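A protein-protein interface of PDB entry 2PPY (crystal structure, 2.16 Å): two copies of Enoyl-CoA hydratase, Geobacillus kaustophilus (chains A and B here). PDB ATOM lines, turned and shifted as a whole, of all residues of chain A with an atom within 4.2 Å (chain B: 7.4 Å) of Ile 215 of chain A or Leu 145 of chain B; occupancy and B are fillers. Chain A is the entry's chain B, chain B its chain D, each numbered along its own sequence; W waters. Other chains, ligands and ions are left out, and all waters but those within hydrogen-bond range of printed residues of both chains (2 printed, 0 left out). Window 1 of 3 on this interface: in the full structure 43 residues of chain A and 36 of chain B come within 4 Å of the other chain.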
ATOM      1  N   ALA A 211     -11.753   8.868 -23.881  1.00  0.00           N
ATOM      2  CA  ALA A 211     -13.115   9.293 -23.583  1.00  0.00           C
ATOM      3  C   ALA A 211     -13.783   8.220 -22.721  1.00  0.00           C
ATOM      4  O   ALA A 211     -14.375   8.517 -21.683  1.00  0.00           O
ATOM      5  CB  ALA A 211     -13.888   9.493 -24.879  1.00  0.00           C
ATOM      6  N   VAL A 212     -13.673   6.969 -23.156  1.00  0.00           N
ATOM      7  CA  VAL A 212     -14.236   5.844 -22.421  1.00  0.00           C
ATOM      8  C   VAL A 212     -13.717   5.854 -20.988  1.00  0.00           C
ATOM      9  O   VAL A 212     -14.457   5.572 -20.044  1.00  0.00           O
ATOM     10  CB  VAL A 212     -13.838   4.497 -23.064  1.00  0.00           C
ATOM     11  CG1 VAL A 212     -14.111   3.353 -22.097  1.00  0.00           C
ATOM     12  CG2 VAL A 212     -14.616   4.281 -24.358  1.00  0.00           C
ATOM     13  N   SER A 213     -12.439   6.181 -20.836  1.00  0.00           N
ATOM     14  CA  SER A 213     -11.808   6.212 -19.528  1.00  0.00           C
ATOM     15  C   SER A 213     -12.333   7.360 -18.659  1.00  0.00           C
ATOM     16  O   SER A 213     -12.701   7.147 -17.504  1.00  0.00           O
ATOM     17  CB  SER A 213     -10.289   6.309 -19.695  1.00  0.00           C
ATOM     18  OG  SER A 213      -9.626   6.198 -18.449  1.00  0.00           O
ATOM     19  N   ASN A 214     -12.380   8.571 -19.209  1.00  0.00           N
ATOM     20  CA  ASN A 214     -12.876   9.713 -18.441  1.00  0.00           C
ATOM     21  C   ASN A 214     -14.364   9.598 -18.131  1.00  0.00           C
ATOM     22  O   ASN A 214     -14.845  10.165 -17.150  1.00  0.00           O
ATOM     23  CB  ASN A 214     -12.594  11.028 -19.173  1.00  0.00           C
ATOM     24  CG  ASN A 214     -11.152  11.470 -19.022  1.00  0.00           C
ATOM     25  OD1 ASN A 214     -10.776  12.570 -19.435  1.00  0.00           O
ATOM     26  ND2 ASN A 214     -10.335  10.612 -18.425  1.00  0.00           N
ATOM     27  N   ILE A 215     -15.089   8.870 -18.975  1.00  0.00           N
ATOM     28  CA  ILE A 215     -16.515   8.662 -18.764  1.00  0.00           C
ATOM     29  C   ILE A 215     -16.682   7.741 -17.556  1.00  0.00           C
ATOM     30  O   ILE A 215     -17.514   7.981 -16.689  1.00  0.00           O
ATOM     31  CB  ILE A 215     -17.163   8.022 -20.005  1.00  0.00           C
ATOM     32  CG1 ILE A 215     -17.296   9.076 -21.112  1.00  0.00           C
ATOM     33  CG2 ILE A 215     -18.504   7.403 -19.635  1.00  0.00           C
ATOM     34  CD1 ILE A 215     -17.619   8.504 -22.504  1.00  0.00           C
ATOM     35  N   LYS A 216     -15.867   6.695 -17.501  1.00  0.00           N
ATOM     36  CA  LYS A 216     -15.898   5.741 -16.398  1.00  0.00           C
ATOM     37  C   LYS A 216     -15.566   6.425 -15.071  1.00  0.00           C
ATOM     38  O   LYS A 216     -16.130   6.089 -14.035  1.00  0.00           O
ATOM     39  CB  LYS A 216     -14.900   4.603 -16.669  1.00  0.00           C
ATOM     40  CG  LYS A 216     -14.730   3.561 -15.548  1.00  0.00           C
ATOM     41  CD  LYS A 216     -13.973   4.132 -14.354  1.00  0.00           C
ATOM     42  CE  LYS A 216     -12.923   3.188 -13.793  1.00  0.00           C
ATOM     43  NZ  LYS A 216     -13.441   1.973 -13.129  1.00  0.00           N
ATOM     44  N   LEU A 217     -14.634   7.373 -15.100  1.00  0.00           N
ATOM     45  CA  LEU A 217     -14.248   8.083 -13.886  1.00  0.00           C
ATOM     46  C   LEU A 217     -15.316   9.097 -13.485  1.00  0.00           C
ATOM     47  O   LEU A 217     -15.629   9.246 -12.310  1.00  0.00           O
ATOM     48  CB  LEU A 217     -12.903   8.796 -14.082  1.00  0.00           C
ATOM     49  CG  LEU A 217     -11.673   7.906 -14.279  1.00  0.00           C
ATOM     50  CD1 LEU A 217     -10.444   8.767 -14.542  1.00  0.00           C
ATOM     51  CD2 LEU A 217     -11.469   7.048 -13.048  1.00  0.00           C
ATOM     52  N   ALA A 218     -15.877   9.786 -14.472  1.00  0.00           N
ATOM     53  CA  ALA A 218     -16.906  10.783 -14.216  1.00  0.00           C
ATOM     54  C   ALA A 218     -18.101  10.158 -13.512  1.00  0.00           C
ATOM     55  O   ALA A 218     -18.611  10.697 -12.529  1.00  0.00           O
ATOM     56  CB  ALA A 218     -17.354  11.424 -15.524  1.00  0.00           C
ATOM     57  N   ILE A 219     -18.539   9.012 -14.013  1.00  0.00           N
ATOM     58  CA  ILE A 219     -19.692   8.341 -13.436  1.00  0.00           C
ATOM     59  C   ILE A 219     -19.440   7.683 -12.082  1.00  0.00           C
ATOM     60  O   ILE A 219     -20.179   7.921 -11.126  1.00  0.00           O
ATOM     61  CB  ILE A 219     -20.245   7.286 -14.417  1.00  0.00           C
ATOM     62  CG1 ILE A 219     -20.828   7.999 -15.644  1.00  0.00           C
ATOM     63  CG2 ILE A 219     -21.294   6.405 -13.727  1.00  0.00           C
ATOM     64  CD1 ILE A 219     -21.377   7.067 -16.719  1.00  0.00           C
ATOM     65  N   GLU A 234     -17.254  16.357 -13.933  1.00  0.00           N
ATOM     66  CA  GLU A 234     -17.518  15.885 -15.286  1.00  0.00           C
ATOM     67  C   GLU A 234     -16.919  16.885 -16.279  1.00  0.00           C
ATOM     68  O   GLU A 234     -16.367  16.502 -17.309  1.00  0.00           O
ATOM     69  CB  GLU A 234     -19.037  15.771 -15.501  1.00  0.00           C
ATOM     70  CG  GLU A 234     -19.489  15.630 -16.958  1.00  0.00           C
ATOM     71  CD  GLU A 234     -20.988  15.870 -17.131  1.00  0.00           C
ATOM     72  OE1 GLU A 234     -21.791  14.959 -16.826  1.00  0.00           O
ATOM     73  OE2 GLU A 234     -21.366  16.981 -17.566  1.00  0.00           O
ATOM     74  N   GLN A 238     -13.974  16.494 -19.114  1.00  0.00           N
ATOM     75  CA  GLN A 238     -14.287  16.875 -20.486  1.00  0.00           C
ATOM     76  C   GLN A 238     -13.209  17.835 -21.025  1.00  0.00           C
ATOM     77  O   GLN A 238     -12.867  17.785 -22.206  1.00  0.00           O
ATOM     78  CB  GLN A 238     -15.661  17.546 -20.554  1.00  0.00           C
ATOM     79  CG  GLN A 238     -16.061  18.040 -21.949  1.00  0.00           C
ATOM     80  CD  GLN A 238     -16.646  16.948 -22.846  1.00  0.00           C
ATOM     81  OE1 GLN A 238     -17.759  17.092 -23.362  1.00  0.00           O
ATOM     82  NE2 GLN A 238     -15.896  15.863 -23.044  1.00  0.00           N
ATOM     83  N   LEU A 241     -10.500  15.932 -22.396  1.00  0.00           N
ATOM     84  CA  LEU A 241     -10.903  15.317 -23.653  1.00  0.00           C
ATOM     85  C   LEU A 241     -10.835  16.302 -24.813  1.00  0.00           C
ATOM     86  O   LEU A 241     -10.406  15.945 -25.911  1.00  0.00           O
ATOM     87  CB  LEU A 241     -12.321  14.758 -23.519  1.00  0.00           C
ATOM     88  CG  LEU A 241     -12.447  13.238 -23.352  1.00  0.00           C
ATOM     89  CD1 LEU A 241     -11.270  12.670 -22.570  1.00  0.00           C
ATOM     90  CD2 LEU A 241     -13.772  12.925 -22.678  1.00  0.00           C
ATOM     91  N   GLU B 118     -29.450  15.394 -22.940  1.00  0.00           N
ATOM     92  CA  GLU B 118     -29.002  16.099 -21.747  1.00  0.00           C
ATOM     93  C   GLU B 118     -30.011  17.177 -21.369  1.00  0.00           C
ATOM     94  O   GLU B 118     -30.324  17.355 -20.189  1.00  0.00           O
ATOM     95  CB  GLU B 118     -27.619  16.705 -21.976  1.00  0.00           C
ATOM     96  CG  GLU B 118     -26.539  15.645 -22.081  1.00  0.00           C
ATOM     97  CD  GLU B 118     -25.176  16.223 -22.363  1.00  0.00           C
ATOM     98  OE1 GLU B 118     -25.026  16.863 -23.428  1.00  0.00           O
ATOM     99  OE2 GLU B 118     -24.260  16.036 -21.525  1.00  0.00           O
ATOM    100  N   LEU B 137     -26.683   8.856 -25.523  1.00  0.00           N
ATOM    101  CA  LEU B 137     -25.550   9.782 -25.539  1.00  0.00           C
ATOM    102  C   LEU B 137     -24.392   9.192 -26.345  1.00  0.00           C
ATOM    103  O   LEU B 137     -23.564   8.456 -25.811  1.00  0.00           O
ATOM    104  CB  LEU B 137     -25.090  10.052 -24.104  1.00  0.00           C
ATOM    105  CG  LEU B 137     -26.178  10.568 -23.154  1.00  0.00           C
ATOM    106  CD1 LEU B 137     -25.700  10.485 -21.711  1.00  0.00           C
ATOM    107  CD2 LEU B 137     -26.546  11.997 -23.530  1.00  0.00           C
ATOM    108  N   PRO B 138     -24.320   9.511 -27.646  1.00  0.00           N
ATOM    109  CA  PRO B 138     -23.251   8.994 -28.507  1.00  0.00           C
ATOM    110  C   PRO B 138     -21.953   9.810 -28.525  1.00  0.00           C
ATOM    111  O   PRO B 138     -21.074   9.569 -29.354  1.00  0.00           O
ATOM    112  CB  PRO B 138     -23.922   8.944 -29.875  1.00  0.00           C
ATOM    113  CG  PRO B 138     -24.792  10.163 -29.845  1.00  0.00           C
ATOM    114  CD  PRO B 138     -25.390  10.138 -28.446  1.00  0.00           C
ATOM    115  N   GLU B 139     -21.825  10.761 -27.607  1.00  0.00           N
ATOM    116  CA  GLU B 139     -20.633  11.603 -27.545  1.00  0.00           C
ATOM    117  C   GLU B 139     -19.292  10.866 -27.638  1.00  0.00           C
ATOM    118  O   GLU B 139     -18.352  11.374 -28.244  1.00  0.00           O
ATOM    119  CB  GLU B 139     -20.647  12.461 -26.272  1.00  0.00           C
ATOM    120  CG  GLU B 139     -21.610  13.636 -26.338  1.00  0.00           C
ATOM    121  CD  GLU B 139     -22.994  13.300 -25.808  1.00  0.00           C
ATOM    122  OE1 GLU B 139     -23.401  12.121 -25.889  1.00  0.00           O
ATOM    123  OE2 GLU B 139     -23.678  14.223 -25.316  1.00  0.00           O
ATOM    124  N   VAL B 140     -19.203   9.680 -27.041  1.00  0.00           N
ATOM    125  CA  VAL B 140     -17.960   8.922 -27.062  1.00  0.00           C
ATOM    126  C   VAL B 140     -17.472   8.649 -28.485  1.00  0.00           C
ATOM    127  O   VAL B 140     -16.266   8.584 -28.729  1.00  0.00           O
ATOM    128  CB  VAL B 140     -18.105   7.576 -26.308  1.00  0.00           C
ATOM    129  CG1 VAL B 140     -19.078   6.657 -27.040  1.00  0.00           C
ATOM    130  CG2 VAL B 140     -16.754   6.910 -26.173  1.00  0.00           C
ATOM    131  N   SER B 141     -18.408   8.499 -29.422  1.00  0.00           N
ATOM    132  CA  SER B 141     -18.050   8.233 -30.814  1.00  0.00           C
ATOM    133  C   SER B 141     -17.320   9.418 -31.447  1.00  0.00           C
ATOM    134  O   SER B 141     -16.866   9.335 -32.586  1.00  0.00           O
ATOM    135  CB  SER B 141     -19.303   7.913 -31.637  1.00  0.00           C
ATOM    136  OG  SER B 141     -20.036   9.092 -31.931  1.00  0.00           O
ATOM    137  N   LEU B 142     -17.216  10.514 -30.701  1.00  0.00           N
ATOM    138  CA  LEU B 142     -16.546  11.725 -31.167  1.00  0.00           C
ATOM    139  C   LEU B 142     -15.289  12.032 -30.349  1.00  0.00           C
ATOM    140  O   LEU B 142     -14.636  13.055 -30.556  1.00  0.00           O
ATOM    141  CB  LEU B 142     -17.495  12.923 -31.083  1.00  0.00           C
ATOM    142  CG  LEU B 142     -18.649  13.034 -32.082  1.00  0.00           C
ATOM    143  CD1 LEU B 142     -19.538  14.196 -31.697  1.00  0.00           C
ATOM    144  CD2 LEU B 142     -18.101  13.239 -33.484  1.00  0.00           C
ATOM    145  N   GLY B 143     -14.957  11.157 -29.409  1.00  0.00           N
ATOM    146  CA  GLY B 143     -13.773  11.388 -28.603  1.00  0.00           C
ATOM    147  C   GLY B 143     -14.004  12.322 -27.429  1.00  0.00           C
ATOM    148  O   GLY B 143     -13.049  12.747 -26.776  1.00  0.00           O
ATOM    149  N   VAL B 144     -15.265  12.668 -27.174  1.00  0.00           N
ATOM    150  CA  VAL B 144     -15.603  13.522 -26.039  1.00  0.00           C
ATOM    151  C   VAL B 144     -16.671  12.800 -25.226  1.00  0.00           C
ATOM    152  O   VAL B 144     -17.049  11.681 -25.564  1.00  0.00           O
ATOM    153  CB  VAL B 144     -16.136  14.916 -26.483  1.00  0.00           C
ATOM    154  CG1 VAL B 144     -15.022  15.702 -27.153  1.00  0.00           C
ATOM    155  CG2 VAL B 144     -17.331  14.763 -27.416  1.00  0.00           C
ATOM    156  N   LEU B 145     -17.147  13.413 -24.149  1.00  0.00           N
ATOM    157  CA  LEU B 145     -18.179  12.776 -23.343  1.00  0.00           C
ATOM    158  C   LEU B 145     -19.395  13.687 -23.240  1.00  0.00           C
ATOM    159  O   LEU B 145     -19.387  14.792 -23.783  1.00  0.00           O
ATOM    160  CB  LEU B 145     -17.632  12.421 -21.950  1.00  0.00           C
ATOM    161  CG  LEU B 145     -17.021  13.490 -21.036  1.00  0.00           C
ATOM    162  CD1 LEU B 145     -18.073  14.507 -20.651  1.00  0.00           C
ATOM    163  CD2 LEU B 145     -16.451  12.827 -19.784  1.00  0.00           C
ATOM    164  N   ALA B 146     -20.449  13.214 -22.579  1.00  0.00           N
ATOM    165  CA  ALA B 146     -21.656  14.018 -22.401  1.00  0.00           C
ATOM    166  C   ALA B 146     -21.329  15.048 -21.316  1.00  0.00           C
ATOM    167  O   ALA B 146     -21.540  14.808 -20.125  1.00  0.00           O
ATOM    168  CB  ALA B 146     -22.822  13.128 -21.971  1.00  0.00           C
ATOM    169  N   GLY B 147     -20.807  16.196 -21.747  1.00  0.00           N
ATOM    170  CA  GLY B 147     -20.395  17.238 -20.822  1.00  0.00           C
ATOM    171  C   GLY B 147     -21.426  18.240 -20.358  1.00  0.00           C
ATOM    172  O   GLY B 147     -21.078  19.194 -19.657  1.00  0.00           O
ATOM    173  N   THR B 148     -22.684  18.050 -20.743  1.00  0.00           N
ATOM    174  CA  THR B 148     -23.738  18.960 -20.313  1.00  0.00           C
ATOM    175  C   THR B 148     -24.591  18.270 -19.246  1.00  0.00           C
ATOM    176  O   THR B 148     -25.821  18.344 -19.271  1.00  0.00           O
ATOM    177  CB  THR B 148     -24.650  19.385 -21.488  1.00  0.00           C
ATOM    178  OG1 THR B 148     -23.851  19.699 -22.634  1.00  0.00           O
ATOM    179  CG2 THR B 148     -25.449  20.623 -21.111  1.00  0.00           C
ATOM    180  N   GLY B 149     -23.926  17.578 -18.321  1.00  0.00           N
ATOM    181  CA  GLY B 149     -24.631  16.902 -17.244  1.00  0.00           C
ATOM    182  C   GLY B 149     -25.085  15.501 -17.579  1.00  0.00           C
ATOM    183  O   GLY B 149     -25.622  14.791 -16.724  1.00  0.00           O
ATOM    184  N   GLY B 150     -24.859  15.102 -18.826  1.00  0.00           N
ATOM    185  CA  GLY B 150     -25.260  13.787 -19.287  1.00  0.00           C
ATOM    186  C   GLY B 150     -24.784  12.596 -18.481  1.00  0.00           C
ATOM    187  O   GLY B 150     -25.585  11.716 -18.167  1.00  0.00           O
ATOM    188  N   THR B 151     -23.497  12.543 -18.151  1.00  0.00           N
ATOM    189  CA  THR B 151     -22.982  11.411 -17.381  1.00  0.00           C
ATOM    190  C   THR B 151     -23.564  11.382 -15.974  1.00  0.00           C
ATOM    191  O   THR B 151     -23.835  10.310 -15.424  1.00  0.00           O
ATOM    192  CB  THR B 151     -21.422  11.429 -17.243  1.00  0.00           C
ATOM    193  OG1 THR B 151     -21.017  12.543 -16.431  1.00  0.00           O
ATOM    194  CG2 THR B 151     -20.749  11.523 -18.617  1.00  0.00           C
ATOM    195  N   GLN B 152     -23.760  12.563 -15.397  1.00  0.00           N
ATOM    196  CA  GLN B 152     -24.269  12.655 -14.035  1.00  0.00           C
ATOM    197  C   GLN B 152     -25.767  12.438 -13.889  1.00  0.00           C
ATOM    198  O   GLN B 152     -26.196  11.674 -13.024  1.00  0.00           O
ATOM    199  CB  GLN B 152     -23.870  13.995 -13.414  1.00  0.00           C
ATOM    200  CG  GLN B 152     -22.351  14.176 -13.303  1.00  0.00           C
ATOM    201  CD  GLN B 152     -21.670  12.959 -12.692  1.00  0.00           C
ATOM    202  OE1 GLN B 152     -21.929  12.594 -11.539  1.00  0.00           O
ATOM    203  NE2 GLN B 152     -20.806  12.317 -13.466  1.00  0.00           N
ATOM    204  N   ALA B 163     -25.946   3.527 -16.778  1.00  0.00           N
ATOM    205  CA  ALA B 163     -25.560   4.794 -17.388  1.00  0.00           C
ATOM    206  C   ALA B 163     -24.128   4.693 -17.921  1.00  0.00           C
ATOM    207  O   ALA B 163     -23.817   5.206 -18.998  1.00  0.00           O
ATOM    208  CB  ALA B 163     -25.668   5.913 -16.373  1.00  0.00           C
ATOM    209  N   LEU B 164     -23.258   4.023 -17.171  1.00  0.00           N
ATOM    210  CA  LEU B 164     -21.875   3.865 -17.598  1.00  0.00           C
ATOM    211  C   LEU B 164     -21.828   3.078 -18.912  1.00  0.00           C
ATOM    212  O   LEU B 164     -21.174   3.488 -19.875  1.00  0.00           O
ATOM    213  CB  LEU B 164     -21.067   3.150 -16.511  1.00  0.00           C
ATOM    214  CG  LEU B 164     -19.577   2.945 -16.806  1.00  0.00           C
ATOM    215  CD1 LEU B 164     -18.772   3.172 -15.538  1.00  0.00           C
ATOM    216  CD2 LEU B 164     -19.344   1.546 -17.350  1.00  0.00           C
ATOM    217  N   ASP B 165     -22.540   1.955 -18.941  1.00  0.00           N
ATOM    218  CA  ASP B 165     -22.618   1.103 -20.124  1.00  0.00           C
ATOM    219  C   ASP B 165     -23.056   1.912 -21.348  1.00  0.00           C
ATOM    220  O   ASP B 165     -22.396   1.876 -22.388  1.00  0.00           O
ATOM    221  CB  ASP B 165     -23.596  -0.047 -19.843  1.00  0.00           C
ATOM    222  CG  ASP B 165     -23.960  -0.847 -21.091  1.00  0.00           C
ATOM    223  OD1 ASP B 165     -23.119  -0.985 -22.009  1.00  0.00           O
ATOM    224  OD2 ASP B 165     -25.100  -1.359 -21.135  1.00  0.00           O
ATOM    225  N   MET B 166     -24.152   2.657 -21.214  1.00  0.00           N
ATOM    226  CA  MET B 166     -24.672   3.470 -22.312  1.00  0.00           C
ATOM    227  C   MET B 166     -23.727   4.587 -22.747  1.00  0.00           C
ATOM    228  O   MET B 166     -23.657   4.925 -23.928  1.00  0.00           O
ATOM    229  CB  MET B 166     -26.024   4.091 -21.937  1.00  0.00           C
ATOM    230  CG  MET B 166     -27.200   3.122 -21.909  1.00  0.00           C
ATOM    231  SD  MET B 166     -28.910   4.037 -21.714  1.00  0.00           S
ATOM    232  CE  MET B 166     -29.031   4.832 -23.461  1.00  0.00           C
ATOM    233  N   ASN B 167     -23.012   5.168 -21.792  1.00  0.00           N
ATOM    234  CA  ASN B 167     -22.086   6.253 -22.099  1.00  0.00           C
ATOM    235  C   ASN B 167     -20.805   5.784 -22.786  1.00  0.00           C
ATOM    236  O   ASN B 167     -20.372   6.379 -23.768  1.00  0.00           O
ATOM    237  CB  ASN B 167     -21.726   7.021 -20.818  1.00  0.00           C
ATOM    238  CG  ASN B 167     -22.724   8.118 -20.493  1.00  0.00           C
ATOM    239  OD1 ASN B 167     -22.639   9.229 -21.026  1.00  0.00           O
ATOM    240  ND2 ASN B 167     -23.686   7.809 -19.627  1.00  0.00           N
ATOM    241  N   ILE B 168     -20.196   4.723 -22.272  1.00  0.00           N
ATOM    242  CA  ILE B 168     -18.957   4.237 -22.866  1.00  0.00           C
ATOM    243  C   ILE B 168     -19.125   3.626 -24.263  1.00  0.00           C
ATOM    244  O   ILE B 168     -18.197   3.672 -25.069  1.00  0.00           O
ATOM    245  CB  ILE B 168     -18.256   3.222 -21.942  1.00  0.00           C
ATOM    246  CG1 ILE B 168     -19.115   1.971 -21.770  1.00  0.00           C
ATOM    247  CG2 ILE B 168     -17.968   3.879 -20.587  1.00  0.00           C
ATOM    248  CD1 ILE B 168     -18.410   0.884 -20.994  1.00  0.00           C
ATOM    249  N   THR B 169     -20.301   3.074 -24.554  1.00  0.00           N
ATOM    250  CA  THR B 169     -20.556   2.471 -25.865  1.00  0.00           C
ATOM    251  C   THR B 169     -21.146   3.493 -26.830  1.00  0.00           C
ATOM    252  O   THR B 169     -20.958   3.392 -28.042  1.00  0.00           O
ATOM    253  CB  THR B 169     -21.537   1.270 -25.781  1.00  0.00           C
ATOM    254  OG1 THR B 169     -22.842   1.736 -25.415  1.00  0.00           O
ATOM    255  CG2 THR B 169     -21.053   0.248 -24.755  1.00  0.00           C
ATOM    256  N   GLY B 170     -21.859   4.474 -26.287  1.00  0.00           N
ATOM    257  CA  GLY B 170     -22.460   5.506 -27.113  1.00  0.00           C
ATOM    258  C   GLY B 170     -23.692   5.043 -27.867  1.00  0.00           C
ATOM    259  O   GLY B 170     -24.196   5.742 -28.753  1.00  0.00           O
HETATM  260  O   HOH W   1     -19.621  19.413 -17.265  1.00  0.00           O
HETATM  261  O   HOH W   2     -22.438   9.898 -11.432  1.00  0.00           O
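Val 140 of chain B touches Val 212 of chain A.
Ile 215 of chain A touches Val 140 of chain B.
Leu 145 of chain B touches Ile 215 of chain A.
Ile 168 of chain B touches Ile 215 of chain A.
Thr 151 of chain B touches Ala 218 of chain A.
Ile 219 of chain A touches Ala 163 of chain B.
Asn 167 of chain B touches Ile 219 of chain A (ND2 to CD1, 3.8 Å).
OE1 of Glu 234 of chain A touches N of Gly 150 of chain B, 3.7 Å away.
Val 144 of chain B touches Leu 241 of chain A (C to CD2, 3.9 Å).
Leu 145 of chain B touches Leu 241 of chain A (CG to CD2, 3.7 Å).
The side-chain carboxylate (OE2) of Glu 118 of chain B lies within hydrogen-bond range of the backbone NH (N) of Gly 147 of chain B (3.5 Å).
The side-chain carboxylate (OE2) of Glu 118 of chain B sits at hydrogen-bond distance from the backbone NH (N) of Thr 148 of chain B.
ND2 of Asn 167 of chain B sits at hydrogen-bond distance from O of Ala 163 of chain B, at 2.7 Å.
The side-chain carboxylate (OE2) of Glu 118 of chain B sits at hydrogen-bond distance from the backbone NH (N) of Gly 150 of chain B (2.9 Å).
OG1 of Thr 151 of chain B sits at hydrogen-bond distance from NE2 of Gln 152 of chain B (3.0 Å).
OE1 of Glu 234 of chain A lies within hydrogen-bond range of OG1 of Thr 151 of chain B, 2.6 Å away.
The side-chain amide nitrogen (NE2) of Gln 152 of chain B sits at hydrogen-bond distance from the backbone carbonyl oxygen (O) of Ala 218 of chain A, at 2.9 Å.
OE1 of Glu 234 of chain A is in hydrogen-bond range of N of Gln 152 of chain B, 3.4 Å away.
OE1 of Glu 234 of chain A lies close to O of Ala 146 of chain B, 3.3 Å away.
O of Gly 147 of chain B lies close to OE2 of Glu 234 of chain A.
OE2 of Glu 234 of chain A is in hydrogen-bond range of N of Gly 149 of chain B (2.7 Å).
The backbone carbonyl oxygen of Leu 145 of chain B lies close to the side-chain amide oxygen of Gln 238 of chain A, 2.8 Å away.
Water W2 lies within hydrogen-bond range of the side-chain amide oxygen of Gln 152 of chain B (2.7 Å) and the backbone carbonyl oxygen of Ile 219 of chain A (3.0 Å).
Water W1 lies within hydrogen-bond range of O of Gly 147 of chain B and OE2 of Glu 234 of chain A.
Of the 25 printed residues of chain B, 15 touch a printed residue of chain A.
Printed residues of chain B that touch a printed residue of chain A: Val 140, Gly 143, Val 144, Leu 145, Ala 146, Gly 147, Thr 148, Gly 149, Gly 150, Thr 151, Gln 152, Ala 163, Leu 164, Asn 167 and Ile 168.
Among the printed residues, 28 pairs touch across the chains.
Asn 214 of chain A touches none of the printed residues of chain B.
Of the printed residues of chain B, Ile 215 of chain A touches Val 140, Leu 145, Asn 167 and Ile 168.
Printed residues of chain B within 4 Å of Glu 234 of chain A: Ala 146, Gly 147, Thr 148, Gly 149, Gly 150, Thr 151 and Gln 152.
Leu 145 of chain B touches just these residues of chain A: Ile 215 (3.5 Å), Gln 238 (2.8 Å) and Leu 241 (3.7 Å).
Of the printed residues of chain A, Thr 148 of chain B touches Glu 234 (3.6 Å).
Of the printed residues of chain A, Gly 150 of chain B touches Glu 234.
Of the printed residues of chain A, Gln 152 of chain B touches Ala 218 (2.9 Å) and Glu 234 (3.4 Å).
No position is printed for both chains.
Of the 28 pairs that touch across the chains among the printed residues, none has its exchanged pair printed and touching as well.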
